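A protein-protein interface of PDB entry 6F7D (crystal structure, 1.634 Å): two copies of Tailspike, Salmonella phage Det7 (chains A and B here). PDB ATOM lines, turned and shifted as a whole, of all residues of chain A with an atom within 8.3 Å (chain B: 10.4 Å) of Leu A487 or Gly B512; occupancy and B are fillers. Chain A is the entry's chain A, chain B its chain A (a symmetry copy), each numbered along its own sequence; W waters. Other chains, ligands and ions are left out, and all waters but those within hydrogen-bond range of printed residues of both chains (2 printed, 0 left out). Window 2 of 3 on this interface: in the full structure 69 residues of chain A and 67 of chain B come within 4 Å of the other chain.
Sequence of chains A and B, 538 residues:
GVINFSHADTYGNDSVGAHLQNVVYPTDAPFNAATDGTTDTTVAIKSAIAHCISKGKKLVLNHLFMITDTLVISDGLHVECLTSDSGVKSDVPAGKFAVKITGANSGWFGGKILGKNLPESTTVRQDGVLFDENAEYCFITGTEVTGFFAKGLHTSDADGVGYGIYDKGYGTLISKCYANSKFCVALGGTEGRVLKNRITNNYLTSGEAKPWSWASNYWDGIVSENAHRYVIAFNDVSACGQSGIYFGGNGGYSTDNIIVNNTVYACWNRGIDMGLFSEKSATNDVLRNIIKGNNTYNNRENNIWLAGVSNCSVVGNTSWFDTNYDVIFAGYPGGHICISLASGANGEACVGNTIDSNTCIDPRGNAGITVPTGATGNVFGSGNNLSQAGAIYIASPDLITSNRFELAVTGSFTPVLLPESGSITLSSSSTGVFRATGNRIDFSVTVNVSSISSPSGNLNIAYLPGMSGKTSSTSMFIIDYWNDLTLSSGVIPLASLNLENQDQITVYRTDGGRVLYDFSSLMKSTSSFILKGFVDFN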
ATOM      1  N   ILE A 479      -7.262   7.895  -0.665  1.00  0.00           N
ATOM      2  CA  ILE A 479      -6.483   7.173   0.324  1.00  0.00           C
ATOM      3  C   ILE A 479      -7.339   5.975   0.712  1.00  0.00           C
ATOM      4  O   ILE A 479      -8.445   6.149   1.242  1.00  0.00           O
ATOM      5  CB  ILE A 479      -6.133   8.067   1.522  1.00  0.00           C
ATOM      6  CG1 ILE A 479      -5.016   9.041   1.116  1.00  0.00           C
ATOM      7  CG2 ILE A 479      -5.635   7.229   2.698  1.00  0.00           C
ATOM      8  CD1 ILE A 479      -5.053  10.313   1.846  1.00  0.00           C
ATOM      9  N   TRP A 482      -5.329   3.230   5.957  1.00  0.00           N
ATOM     10  CA  TRP A 482      -4.517   3.967   6.927  1.00  0.00           C
ATOM     11  C   TRP A 482      -4.535   3.234   8.256  1.00  0.00           C
ATOM     12  O   TRP A 482      -5.364   2.352   8.499  1.00  0.00           O
ATOM     13  CB  TRP A 482      -4.993   5.394   7.146  1.00  0.00           C
ATOM     14  CG  TRP A 482      -6.425   5.474   7.555  1.00  0.00           C
ATOM     15  CD1 TRP A 482      -6.922   5.488   8.846  1.00  0.00           C
ATOM     16  CD2 TRP A 482      -7.561   5.566   6.684  1.00  0.00           C
ATOM     17  NE1 TRP A 482      -8.294   5.592   8.810  1.00  0.00           N
ATOM     18  CE2 TRP A 482      -8.712   5.637   7.501  1.00  0.00           C
ATOM     19  CE3 TRP A 482      -7.716   5.594   5.291  1.00  0.00           C
ATOM     20  CZ2 TRP A 482     -10.000   5.759   6.972  1.00  0.00           C
ATOM     21  CZ3 TRP A 482      -8.998   5.704   4.766  1.00  0.00           C
ATOM     22  CH2 TRP A 482     -10.124   5.784   5.605  1.00  0.00           C
ATOM     23  N   ASN A 483      -3.607   3.648   9.115  1.00  0.00           N
ATOM     24  CA  ASN A 483      -3.408   3.034  10.415  1.00  0.00           C
ATOM     25  C   ASN A 483      -2.760   4.055  11.334  1.00  0.00           C
ATOM     26  O   ASN A 483      -1.856   4.784  10.915  1.00  0.00           O
ATOM     27  CB  ASN A 483      -2.526   1.790  10.316  1.00  0.00           C
ATOM     28  CG  ASN A 483      -2.591   0.933  11.570  1.00  0.00           C
ATOM     29  OD1 ASN A 483      -3.683   0.543  12.021  1.00  0.00           O
ATOM     30  ND2 ASN A 483      -1.432   0.637  12.139  1.00  0.00           N
ATOM     31  N   ASP A 484      -3.216   4.080  12.594  1.00  0.00           N
ATOM     32  CA  ASP A 484      -2.620   4.913  13.647  1.00  0.00           C
ATOM     33  C   ASP A 484      -2.635   6.388  13.282  1.00  0.00           C
ATOM     34  O   ASP A 484      -1.675   7.130  13.524  1.00  0.00           O
ATOM     35  CB  ASP A 484      -1.203   4.456  13.983  1.00  0.00           C
ATOM     36  CG  ASP A 484      -1.191   3.307  14.967  1.00  0.00           C
ATOM     37  OD1 ASP A 484      -2.276   2.929  15.465  1.00  0.00           O
ATOM     38  OD2 ASP A 484      -0.099   2.776  15.234  1.00  0.00           O
ATOM     39  N   LEU A 485      -3.727   6.830  12.684  1.00  0.00           N
ATOM     40  CA  LEU A 485      -3.962   8.250  12.568  1.00  0.00           C
ATOM     41  C   LEU A 485      -4.846   8.703  13.729  1.00  0.00           C
ATOM     42  O   LEU A 485      -5.619   7.926  14.300  1.00  0.00           O
ATOM     43  CB  LEU A 485      -4.618   8.565  11.228  1.00  0.00           C
ATOM     44  CG  LEU A 485      -3.743   8.298   9.998  1.00  0.00           C
ATOM     45  CD1 LEU A 485      -4.618   8.574   8.743  1.00  0.00           C
ATOM     46  CD2 LEU A 485      -2.522   9.187  10.037  1.00  0.00           C
ATOM     47  N   THR A 486      -4.736   9.980  14.070  1.00  0.00           N
ATOM     48  CA  THR A 486      -5.607  10.576  15.081  1.00  0.00           C
ATOM     49  C   THR A 486      -6.839  11.161  14.386  1.00  0.00           C
ATOM     50  O   THR A 486      -6.919  12.354  14.085  1.00  0.00           O
ATOM     51  CB  THR A 486      -4.853  11.639  15.869  1.00  0.00           C
ATOM     52  OG1 THR A 486      -3.632  11.082  16.356  1.00  0.00           O
ATOM     53  CG2 THR A 486      -5.695  12.106  17.047  1.00  0.00           C
ATOM     54  N   LEU A 487      -7.809  10.290  14.100  1.00  0.00           N
ATOM     55  CA  LEU A 487      -9.022  10.693  13.402  1.00  0.00           C
ATOM     56  C   LEU A 487     -10.235  10.337  14.243  1.00  0.00           C
ATOM     57  O   LEU A 487     -10.399   9.179  14.640  1.00  0.00           O
ATOM     58  CB  LEU A 487      -9.153  10.008  12.036  1.00  0.00           C
ATOM     59  CG  LEU A 487      -8.032  10.128  11.013  1.00  0.00           C
ATOM     60  CD1 LEU A 487      -8.447   9.394   9.739  1.00  0.00           C
ATOM     61  CD2 LEU A 487      -7.749  11.588  10.716  1.00  0.00           C
ATOM     62  N   SER A 488     -11.098  11.319  14.474  1.00  0.00           N
ATOM     63  CA  SER A 488     -12.368  11.026  15.116  1.00  0.00           C
ATOM     64  C   SER A 488     -13.212  10.125  14.225  1.00  0.00           C
ATOM     65  O   SER A 488     -12.958   9.966  13.025  1.00  0.00           O
ATOM     66  CB  SER A 488     -13.127  12.316  15.424  1.00  0.00           C
ATOM     67  OG  SER A 488     -12.363  13.127  16.288  1.00  0.00           O
ATOM     68  N   SER A 489     -14.218   9.508  14.834  1.00  0.00           N
ATOM     69  CA  SER A 489     -15.152   8.705  14.066  1.00  0.00           C
ATOM     70  C   SER A 489     -15.804   9.573  12.997  1.00  0.00           C
ATOM     71  O   SER A 489     -16.186  10.720  13.251  1.00  0.00           O
ATOM     72  CB  SER A 489     -16.207   8.090  14.994  1.00  0.00           C
ATOM     73  OG  SER A 489     -17.436   7.879  14.317  1.00  0.00           O
ATOM     74  N   GLY A 490     -15.895   9.032  11.779  1.00  0.00           N
ATOM     75  CA  GLY A 490     -16.490   9.746  10.667  1.00  0.00           C
ATOM     76  C   GLY A 490     -15.581  10.712   9.939  1.00  0.00           C
ATOM     77  O   GLY A 490     -16.006  11.290   8.929  1.00  0.00           O
ATOM     78  N   VAL A 491     -14.359  10.923  10.415  1.00  0.00           N
ATOM     79  CA  VAL A 491     -13.387  11.761   9.723  1.00  0.00           C
ATOM     80  C   VAL A 491     -12.577  10.842   8.810  1.00  0.00           C
ATOM     81  O   VAL A 491     -12.012   9.838   9.268  1.00  0.00           O
ATOM     82  CB  VAL A 491     -12.485  12.510  10.718  1.00  0.00           C
ATOM     83  CG1 VAL A 491     -11.485  13.406   9.991  1.00  0.00           C
ATOM     84  CG2 VAL A 491     -13.323  13.346  11.682  1.00  0.00           C
ATOM     85  N   ILE A 492     -12.573  11.135   7.509  1.00  0.00           N
ATOM     86  CA  ILE A 492     -11.799  10.295   6.587  1.00  0.00           C
ATOM     87  C   ILE A 492     -10.766  11.139   5.850  1.00  0.00           C
ATOM     88  O   ILE A 492     -10.974  12.348   5.645  1.00  0.00           O
ATOM     89  CB  ILE A 492     -12.710   9.535   5.607  1.00  0.00           C
ATOM     90  CG1 ILE A 492     -13.267  10.465   4.546  1.00  0.00           C
ATOM     91  CG2 ILE A 492     -13.833   8.771   6.372  1.00  0.00           C
ATOM     92  CD1 ILE A 492     -13.694   9.736   3.267  1.00  0.00           C
ATOM     93  N   PRO A 493      -9.629  10.547   5.475  1.00  0.00           N
ATOM     94  CA  PRO A 493      -8.601  11.298   4.742  1.00  0.00           C
ATOM     95  C   PRO A 493      -9.023  11.534   3.297  1.00  0.00           C
ATOM     96  O   PRO A 493      -9.701  10.704   2.680  1.00  0.00           O
ATOM     97  CB  PRO A 493      -7.365  10.387   4.810  1.00  0.00           C
ATOM     98  CG  PRO A 493      -7.696   9.301   5.719  1.00  0.00           C
ATOM     99  CD  PRO A 493      -9.183   9.195   5.834  1.00  0.00           C
ATOM    100  N   LEU A 494      -8.609  12.688   2.775  1.00  0.00           N
ATOM    101  CA  LEU A 494      -8.837  13.109   1.401  1.00  0.00           C
ATOM    102  C   LEU A 494      -7.490  13.475   0.797  1.00  0.00           C
ATOM    103  O   LEU A 494      -6.549  13.829   1.519  1.00  0.00           O
ATOM    104  CB  LEU A 494      -9.774  14.322   1.303  1.00  0.00           C
ATOM    105  CG  LEU A 494     -11.187  14.170   1.853  1.00  0.00           C
ATOM    106  CD1 LEU A 494     -11.882  15.522   1.880  1.00  0.00           C
ATOM    107  CD2 LEU A 494     -11.968  13.178   1.003  1.00  0.00           C
ATOM    108  N   TYR A 508      -5.474  15.815   3.375  1.00  0.00           N
ATOM    109  CA  TYR A 508      -6.298  16.542   4.348  1.00  0.00           C
ATOM    110  C   TYR A 508      -7.484  15.666   4.759  1.00  0.00           C
ATOM    111  O   TYR A 508      -7.505  14.452   4.519  1.00  0.00           O
ATOM    112  CB  TYR A 508      -6.715  17.899   3.770  1.00  0.00           C
ATOM    113  CG  TYR A 508      -7.342  17.840   2.384  1.00  0.00           C
ATOM    114  CD1 TYR A 508      -6.549  17.672   1.232  1.00  0.00           C
ATOM    115  CD2 TYR A 508      -8.710  17.938   2.225  1.00  0.00           C
ATOM    116  CE1 TYR A 508      -7.116  17.621  -0.026  1.00  0.00           C
ATOM    117  CE2 TYR A 508      -9.288  17.890   0.963  1.00  0.00           C
ATOM    118  CZ  TYR A 508      -8.484  17.733  -0.159  1.00  0.00           C
ATOM    119  OH  TYR A 508      -9.069  17.695  -1.403  1.00  0.00           O
ATOM    120  N   ARG A 509      -8.473  16.254   5.438  1.00  0.00           N
ATOM    121  CA  ARG A 509      -9.519  15.382   5.942  1.00  0.00           C
ATOM    122  C   ARG A 509     -10.842  16.121   6.049  1.00  0.00           C
ATOM    123  O   ARG A 509     -10.910  17.341   5.918  1.00  0.00           O
ATOM    124  CB  ARG A 509      -9.124  14.757   7.285  1.00  0.00           C
ATOM    125  CG  ARG A 509      -8.611  15.751   8.305  1.00  0.00           C
ATOM    126  CD  ARG A 509      -9.737  16.544   8.910  1.00  0.00           C
ATOM    127  NE  ARG A 509      -9.349  17.200  10.150  1.00  0.00           N
ATOM    128  CZ  ARG A 509     -10.166  17.347  11.184  1.00  0.00           C
ATOM    129  NH1 ARG A 509     -11.420  16.889  11.114  1.00  0.00           N
ATOM    130  NH2 ARG A 509      -9.730  17.957  12.276  1.00  0.00           N
ATOM    131  N   THR A 510     -11.890  15.346   6.318  1.00  0.00           N
ATOM    132  CA  THR A 510     -13.257  15.843   6.365  1.00  0.00           C
ATOM    133  C   THR A 510     -13.589  16.390   7.744  1.00  0.00           C
ATOM    134  O   THR A 510     -13.007  15.984   8.750  1.00  0.00           O
ATOM    135  CB  THR A 510     -14.272  14.752   6.029  1.00  0.00           C
ATOM    136  OG1 THR A 510     -14.201  13.690   6.989  1.00  0.00           O
ATOM    137  CG2 THR A 510     -14.018  14.168   4.628  1.00  0.00           C
ATOM    138  N   ASP A 518      -5.356  20.131   8.317  1.00  0.00           N
ATOM    139  CA  ASP A 518      -4.538  20.017   9.526  1.00  0.00           C
ATOM    140  C   ASP A 518      -3.946  18.623   9.684  1.00  0.00           C
ATOM    141  O   ASP A 518      -3.678  18.178  10.806  1.00  0.00           O
ATOM    142  CB  ASP A 518      -5.365  20.374  10.764  1.00  0.00           C
ATOM    143  CG  ASP A 518      -6.605  19.491  10.929  1.00  0.00           C
ATOM    144  OD1 ASP A 518      -6.878  18.632  10.070  1.00  0.00           O
ATOM    145  OD2 ASP A 518      -7.312  19.641  11.948  1.00  0.00           O
ATOM    146  N   PHE A 519      -3.746  17.916   8.563  1.00  0.00           N
ATOM    147  CA  PHE A 519      -3.463  16.487   8.639  1.00  0.00           C
ATOM    148  C   PHE A 519      -2.150  16.199   9.359  1.00  0.00           C
ATOM    149  O   PHE A 519      -2.014  15.143  10.003  1.00  0.00           O
ATOM    150  CB  PHE A 519      -3.457  15.894   7.224  1.00  0.00           C
ATOM    151  CG  PHE A 519      -3.839  14.444   7.171  1.00  0.00           C
ATOM    152  CD1 PHE A 519      -2.870  13.462   7.302  1.00  0.00           C
ATOM    153  CD2 PHE A 519      -5.162  14.059   6.978  1.00  0.00           C
ATOM    154  CE1 PHE A 519      -3.190  12.110   7.248  1.00  0.00           C
ATOM    155  CE2 PHE A 519      -5.497  12.709   6.928  1.00  0.00           C
ATOM    156  CZ  PHE A 519      -4.495  11.727   7.058  1.00  0.00           C
ATOM    157  N   SER A 521      -1.104  17.438  11.951  1.00  0.00           N
ATOM    158  CA  SER A 521      -1.447  17.381  13.365  1.00  0.00           C
ATOM    159  C   SER A 521      -2.061  16.054  13.761  1.00  0.00           C
ATOM    160  O   SER A 521      -2.132  15.760  14.958  1.00  0.00           O
ATOM    161  CB  SER A 521      -2.415  18.512  13.711  1.00  0.00           C
ATOM    162  OG  SER A 521      -1.786  19.769  13.530  1.00  0.00           O
ATOM    163  N   LEU A 522      -2.495  15.246  12.798  1.00  0.00           N
ATOM    164  CA  LEU A 522      -3.141  13.971  13.076  1.00  0.00           C
ATOM    165  C   LEU A 522      -2.193  12.796  12.899  1.00  0.00           C
ATOM    166  O   LEU A 522      -2.608  11.640  13.070  1.00  0.00           O
ATOM    167  CB  LEU A 522      -4.379  13.817  12.180  1.00  0.00           C
ATOM    168  CG  LEU A 522      -5.241  15.095  12.161  1.00  0.00           C
ATOM    169  CD1 LEU A 522      -6.374  15.025  11.137  1.00  0.00           C
ATOM    170  CD2 LEU A 522      -5.798  15.426  13.575  1.00  0.00           C
ATOM    171  N   MET A 523      -0.927  13.070  12.582  1.00  0.00           N
ATOM    172  CA  MET A 523       0.077  12.046  12.337  1.00  0.00           C
ATOM    173  C   MET A 523       0.752  11.660  13.647  1.00  0.00           C
ATOM    174  O   MET A 523       0.959  12.506  14.518  1.00  0.00           O
ATOM    175  CB  MET A 523       1.122  12.559  11.343  1.00  0.00           C
ATOM    176  CG  MET A 523       0.538  13.012  10.002  1.00  0.00           C
ATOM    177  SD  MET A 523       0.073  11.600   8.972  1.00  0.00           S
ATOM    178  CE  MET A 523       1.635  10.870   8.565  1.00  0.00           C
ATOM    179  N   LYS A 524       1.075  10.380  13.785  1.00  0.00           N
ATOM    180  CA  LYS A 524       1.883   9.859  14.875  1.00  0.00           C
ATOM    181  C   LYS A 524       3.134   9.208  14.312  1.00  0.00           C
ATOM    182  O   LYS A 524       3.271   8.996  13.101  1.00  0.00           O
ATOM    183  CB  LYS A 524       1.129   8.821  15.713  1.00  0.00           C
ATOM    184  CG  LYS A 524      -0.272   9.178  16.106  1.00  0.00           C
ATOM    185  CD  LYS A 524      -0.893   7.985  16.790  1.00  0.00           C
ATOM    186  CE  LYS A 524      -2.344   8.223  17.101  1.00  0.00           C
ATOM    187  NZ  LYS A 524      -2.886   7.091  17.887  1.00  0.00           N
ATOM    188  N   SER B 488     -22.245   1.557  11.196  1.00  0.00           N
ATOM    189  CA  SER B 488     -22.514   2.699  12.053  1.00  0.00           C
ATOM    190  C   SER B 488     -22.351   3.994  11.267  1.00  0.00           C
ATOM    191  O   SER B 488     -21.767   4.032  10.179  1.00  0.00           O
ATOM    192  CB  SER B 488     -21.575   2.699  13.259  1.00  0.00           C
ATOM    193  OG  SER B 488     -21.761   1.521  14.011  1.00  0.00           O
ATOM    194  N   SER B 489     -22.902   5.066  11.824  1.00  0.00           N
ATOM    195  CA  SER B 489     -22.726   6.373  11.220  1.00  0.00           C
ATOM    196  C   SER B 489     -21.237   6.691  11.129  1.00  0.00           C
ATOM    197  O   SER B 489     -20.472   6.440  12.067  1.00  0.00           O
ATOM    198  CB  SER B 489     -23.465   7.439  12.037  1.00  0.00           C
ATOM    199  OG  SER B 489     -22.840   8.708  11.926  1.00  0.00           O
ATOM    200  N   GLY B 490     -20.820   7.210   9.973  1.00  0.00           N
ATOM    201  CA  GLY B 490     -19.430   7.558   9.746  1.00  0.00           C
ATOM    202  C   GLY B 490     -18.526   6.421   9.320  1.00  0.00           C
ATOM    203  O   GLY B 490     -17.348   6.670   9.032  1.00  0.00           O
ATOM    204  N   VAL B 491     -19.020   5.189   9.282  1.00  0.00           N
ATOM    205  CA  VAL B 491     -18.248   4.054   8.791  1.00  0.00           C
ATOM    206  C   VAL B 491     -18.547   3.926   7.298  1.00  0.00           C
ATOM    207  O   VAL B 491     -19.717   3.842   6.895  1.00  0.00           O
ATOM    208  CB  VAL B 491     -18.602   2.766   9.553  1.00  0.00           C
ATOM    209  CG1 VAL B 491     -17.773   1.584   9.052  1.00  0.00           C
ATOM    210  CG2 VAL B 491     -18.386   2.949  11.052  1.00  0.00           C
ATOM    211  N   ILE B 492     -17.505   3.982   6.467  1.00  0.00           N
ATOM    212  CA  ILE B 492     -17.731   3.849   5.023  1.00  0.00           C
ATOM    213  C   ILE B 492     -16.943   2.665   4.476  1.00  0.00           C
ATOM    214  O   ILE B 492     -15.888   2.303   5.027  1.00  0.00           O
ATOM    215  CB  ILE B 492     -17.394   5.148   4.271  1.00  0.00           C
ATOM    216  CG1 ILE B 492     -15.894   5.351   4.180  1.00  0.00           C
ATOM    217  CG2 ILE B 492     -18.117   6.367   4.918  1.00  0.00           C
ATOM    218  CD1 ILE B 492     -15.476   6.261   3.019  1.00  0.00           C
ATOM    219  N   LEU B 494     -14.466   0.527   2.066  1.00  0.00           N
ATOM    220  CA  LEU B 494     -13.221   0.734   1.342  1.00  0.00           C
ATOM    221  C   LEU B 494     -12.947  -0.515   0.520  1.00  0.00           C
ATOM    222  O   LEU B 494     -13.419  -1.610   0.857  1.00  0.00           O
ATOM    223  CB  LEU B 494     -12.030   0.986   2.278  1.00  0.00           C
ATOM    224  CG  LEU B 494     -12.097   2.201   3.196  1.00  0.00           C
ATOM    225  CD1 LEU B 494     -10.953   2.159   4.196  1.00  0.00           C
ATOM    226  CD2 LEU B 494     -12.044   3.477   2.369  1.00  0.00           C
ATOM    227  N   ARG B 509     -13.658  -1.686   5.845  1.00  0.00           N
ATOM    228  CA  ARG B 509     -14.313  -0.441   6.208  1.00  0.00           C
ATOM    229  C   ARG B 509     -13.486   0.339   7.214  1.00  0.00           C
ATOM    230  O   ARG B 509     -12.508  -0.160   7.769  1.00  0.00           O
ATOM    231  CB  ARG B 509     -15.731  -0.693   6.736  1.00  0.00           C
ATOM    232  CG  ARG B 509     -15.817  -1.764   7.802  1.00  0.00           C
ATOM    233  CD  ARG B 509     -15.322  -1.255   9.128  1.00  0.00           C
ATOM    234  NE  ARG B 509     -15.756  -2.091  10.238  1.00  0.00           N
ATOM    235  CZ  ARG B 509     -16.085  -1.609  11.429  1.00  0.00           C
ATOM    236  NH1 ARG B 509     -16.017  -0.293  11.659  1.00  0.00           N
ATOM    237  NH2 ARG B 509     -16.470  -2.443  12.384  1.00  0.00           N
ATOM    238  N   THR B 510     -13.919   1.575   7.450  1.00  0.00           N
ATOM    239  CA  THR B 510     -13.213   2.517   8.305  1.00  0.00           C
ATOM    240  C   THR B 510     -13.613   2.336   9.760  1.00  0.00           C
ATOM    241  O   THR B 510     -14.709   1.872  10.069  1.00  0.00           O
ATOM    242  CB  THR B 510     -13.496   3.966   7.910  1.00  0.00           C
ATOM    243  OG1 THR B 510     -14.891   4.261   8.059  1.00  0.00           O
ATOM    244  CG2 THR B 510     -13.086   4.235   6.451  1.00  0.00           C
ATOM    245  N   ASP B 511     -12.713   2.744  10.649  1.00  0.00           N
ATOM    246  CA  ASP B 511     -12.948   2.740  12.097  1.00  0.00           C
ATOM    247  C   ASP B 511     -12.064   3.853  12.674  1.00  0.00           C
ATOM    248  O   ASP B 511     -11.011   3.616  13.266  1.00  0.00           O
ATOM    249  CB  ASP B 511     -12.642   1.375  12.716  1.00  0.00           C
ATOM    250  CG  ASP B 511     -12.819   1.373  14.245  1.00  0.00           C
ATOM    251  OD1 ASP B 511     -13.799   1.964  14.716  1.00  0.00           O
ATOM    252  OD2 ASP B 511     -11.974   0.805  14.960  1.00  0.00           O
ATOM    253  N   GLY B 512     -12.472   5.103  12.441  1.00  0.00           N
ATOM    254  CA  GLY B 512     -11.695   6.229  12.944  1.00  0.00           C
ATOM    255  C   GLY B 512     -10.314   6.272  12.307  1.00  0.00           C
ATOM    256  O   GLY B 512     -10.183   6.325  11.077  1.00  0.00           O
ATOM    257  N   GLY B 513      -9.267   6.230  13.142  1.00  0.00           N
ATOM    258  CA  GLY B 513      -7.877   6.280  12.719  1.00  0.00           C
ATOM    259  C   GLY B 513      -7.287   4.977  12.226  1.00  0.00           C
ATOM    260  O   GLY B 513      -6.076   4.878  12.023  1.00  0.00           O
ATOM    261  N   ARG B 514      -8.107   3.953  12.020  1.00  0.00           N
ATOM    262  CA  ARG B 514      -7.640   2.697  11.458  1.00  0.00           C
ATOM    263  C   ARG B 514      -8.738   2.168  10.552  1.00  0.00           C
ATOM    264  O   ARG B 514      -9.798   2.787  10.403  1.00  0.00           O
ATOM    265  CB  ARG B 514      -7.306   1.679  12.552  1.00  0.00           C
ATOM    266  CG  ARG B 514      -8.537   1.276  13.337  1.00  0.00           C
ATOM    267  CD  ARG B 514      -8.278   0.117  14.261  1.00  0.00           C
ATOM    268  NE  ARG B 514      -9.475  -0.174  15.045  1.00  0.00           N
ATOM    269  CZ  ARG B 514      -9.535  -1.098  15.999  1.00  0.00           C
ATOM    270  NH1 ARG B 514      -8.465  -1.824  16.279  1.00  0.00           N
ATOM    271  NH2 ARG B 514     -10.668  -1.300  16.665  1.00  0.00           N
ATOM    272  N   VAL B 515      -8.482   1.007   9.941  1.00  0.00           N
ATOM    273  CA  VAL B 515      -9.483   0.316   9.153  1.00  0.00           C
ATOM    274  C   VAL B 515      -9.688  -1.065   9.757  1.00  0.00           C
ATOM    275  O   VAL B 515      -8.861  -1.574  10.521  1.00  0.00           O
ATOM    276  CB  VAL B 515      -9.102   0.220   7.650  1.00  0.00           C
ATOM    277  CG1 VAL B 515      -8.790   1.593   7.090  1.00  0.00           C
ATOM    278  CG2 VAL B 515      -7.910  -0.725   7.444  1.00  0.00           C
ATOM    279  N   LEU B 516     -10.817  -1.665   9.427  1.00  0.00           N
ATOM    280  CA  LEU B 516     -11.152  -2.974   9.958  1.00  0.00           C
ATOM    281  C   LEU B 516     -11.542  -3.910   8.830  1.00  0.00           C
ATOM    282  O   LEU B 516     -12.294  -3.533   7.926  1.00  0.00           O
ATOM    283  CB  LEU B 516     -12.297  -2.881  10.984  1.00  0.00           C
ATOM    284  CG  LEU B 516     -11.906  -2.380  12.389  1.00  0.00           C
ATOM    285  CD1 LEU B 516     -13.138  -2.437  13.285  1.00  0.00           C
ATOM    286  CD2 LEU B 516     -10.749  -3.181  12.998  1.00  0.00           C
HETATM  287  O   HOH W   1     -12.246   7.148   9.594  1.00  0.00           O
HETATM  288  O   HOH W   2      -5.516   0.217  10.103  1.00  0.00           O
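The backbone carbonyl oxygen (O) of Gly B512 lies within hydrogen-bond range of the indole nitrogen (NE1) of Trp A482, at 3.0 Å.
O of Gly B513 sits at hydrogen-bond distance from N of Asp A484.
O of Gly B513 is in hydrogen-bond range of N of Leu A485 (3.1 Å).
O of Leu A487 lies within hydrogen-bond range of N of Gly B513.
The side-chain hydroxyl (OG1) of Thr A510 sits at hydrogen-bond distance from the backbone NH (N) of Ile A492, at 3.1 Å.
N of Ile B492 is in hydrogen-bond range of OG1 of Thr B510, at 3.1 Å.
The side-chain carboxylate of Asp B511 lies within salt-bridge range of the guanidinium group of Arg B514, 2.7 Å away.
Among the printed residues, pairs that only touch across the chains: Trp A482 with Gly B513, Trp A482 with Thr B510, Asn A483 with Gly B513, Trp A482 with Arg B514, Gly A490 with Gly B490, Leu A487 with Gly B512, Trp A482 with Val B515, Asn A483 with Arg B514, Ile A492 with Ile B492, Ser A488 with Gly B512 and Trp A482 with Leu B494.
Printed residues of chain B within 4 Å of Asn A483: Gly B513 and Arg B514.
Of chain B, only Gly B512 and Gly B513 come within 4 Å of Leu A487.
Ser A488 touches one residue of chain B.
Ser A489 touches none of the printed residues of chain B.
No residue of chain B comes within 4 Å of Val A491.
Of the printed residues of chain B, Ile A492 touches Ile B492.
Met A523 touches none of the printed residues of chain B.
Of the printed residues of chain A, Thr B510 touches Trp A482.
Gly B512 touches just these residues of chain A: Trp A482 (3.0 Å), Leu A487 (3.6 Å) and Ser A488 (3.9 Å).
Of the printed residues of chain A, Gly B513 touches Trp A482, Asn A483, Asp A484, Leu A485 and Leu A487.
Of the 14 printed residues of chain B, 8 touch a printed residue of chain A.
Printed residues of chain B that touch a printed residue of chain A: Gly B490, Ile B492, Leu B494, Thr B510, Gly B512, Gly B513, Arg B514 and Val B515.
Of the 23 printed residues of chain A, 8 touch a printed residue of chain B.
Hydrophobic or aromatic side chains of chain A within 4 Å of the printed part of chain B: Trp A482, Leu A487 and Ile A492.
Among the printed residues, 15 pairs touch across the chains.
Gly A490 touches its own counterpart, Gly B490.
Ile A492 touches its own counterpart, Ile B492.
Of the 15 pairs that touch across the chains among the printed residues, 2 have their exchanged pair printed and touching as well.
Water W1 bridges the backbone carbonyl oxygen of Gly B512 (2.7 Å) and the backbone carbonyl oxygen of Val A491 (2.7 Å).
Water W2 lies within hydrogen-bond range of OD1 of Asn A483, O of Trp A482 and N of Val B515.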
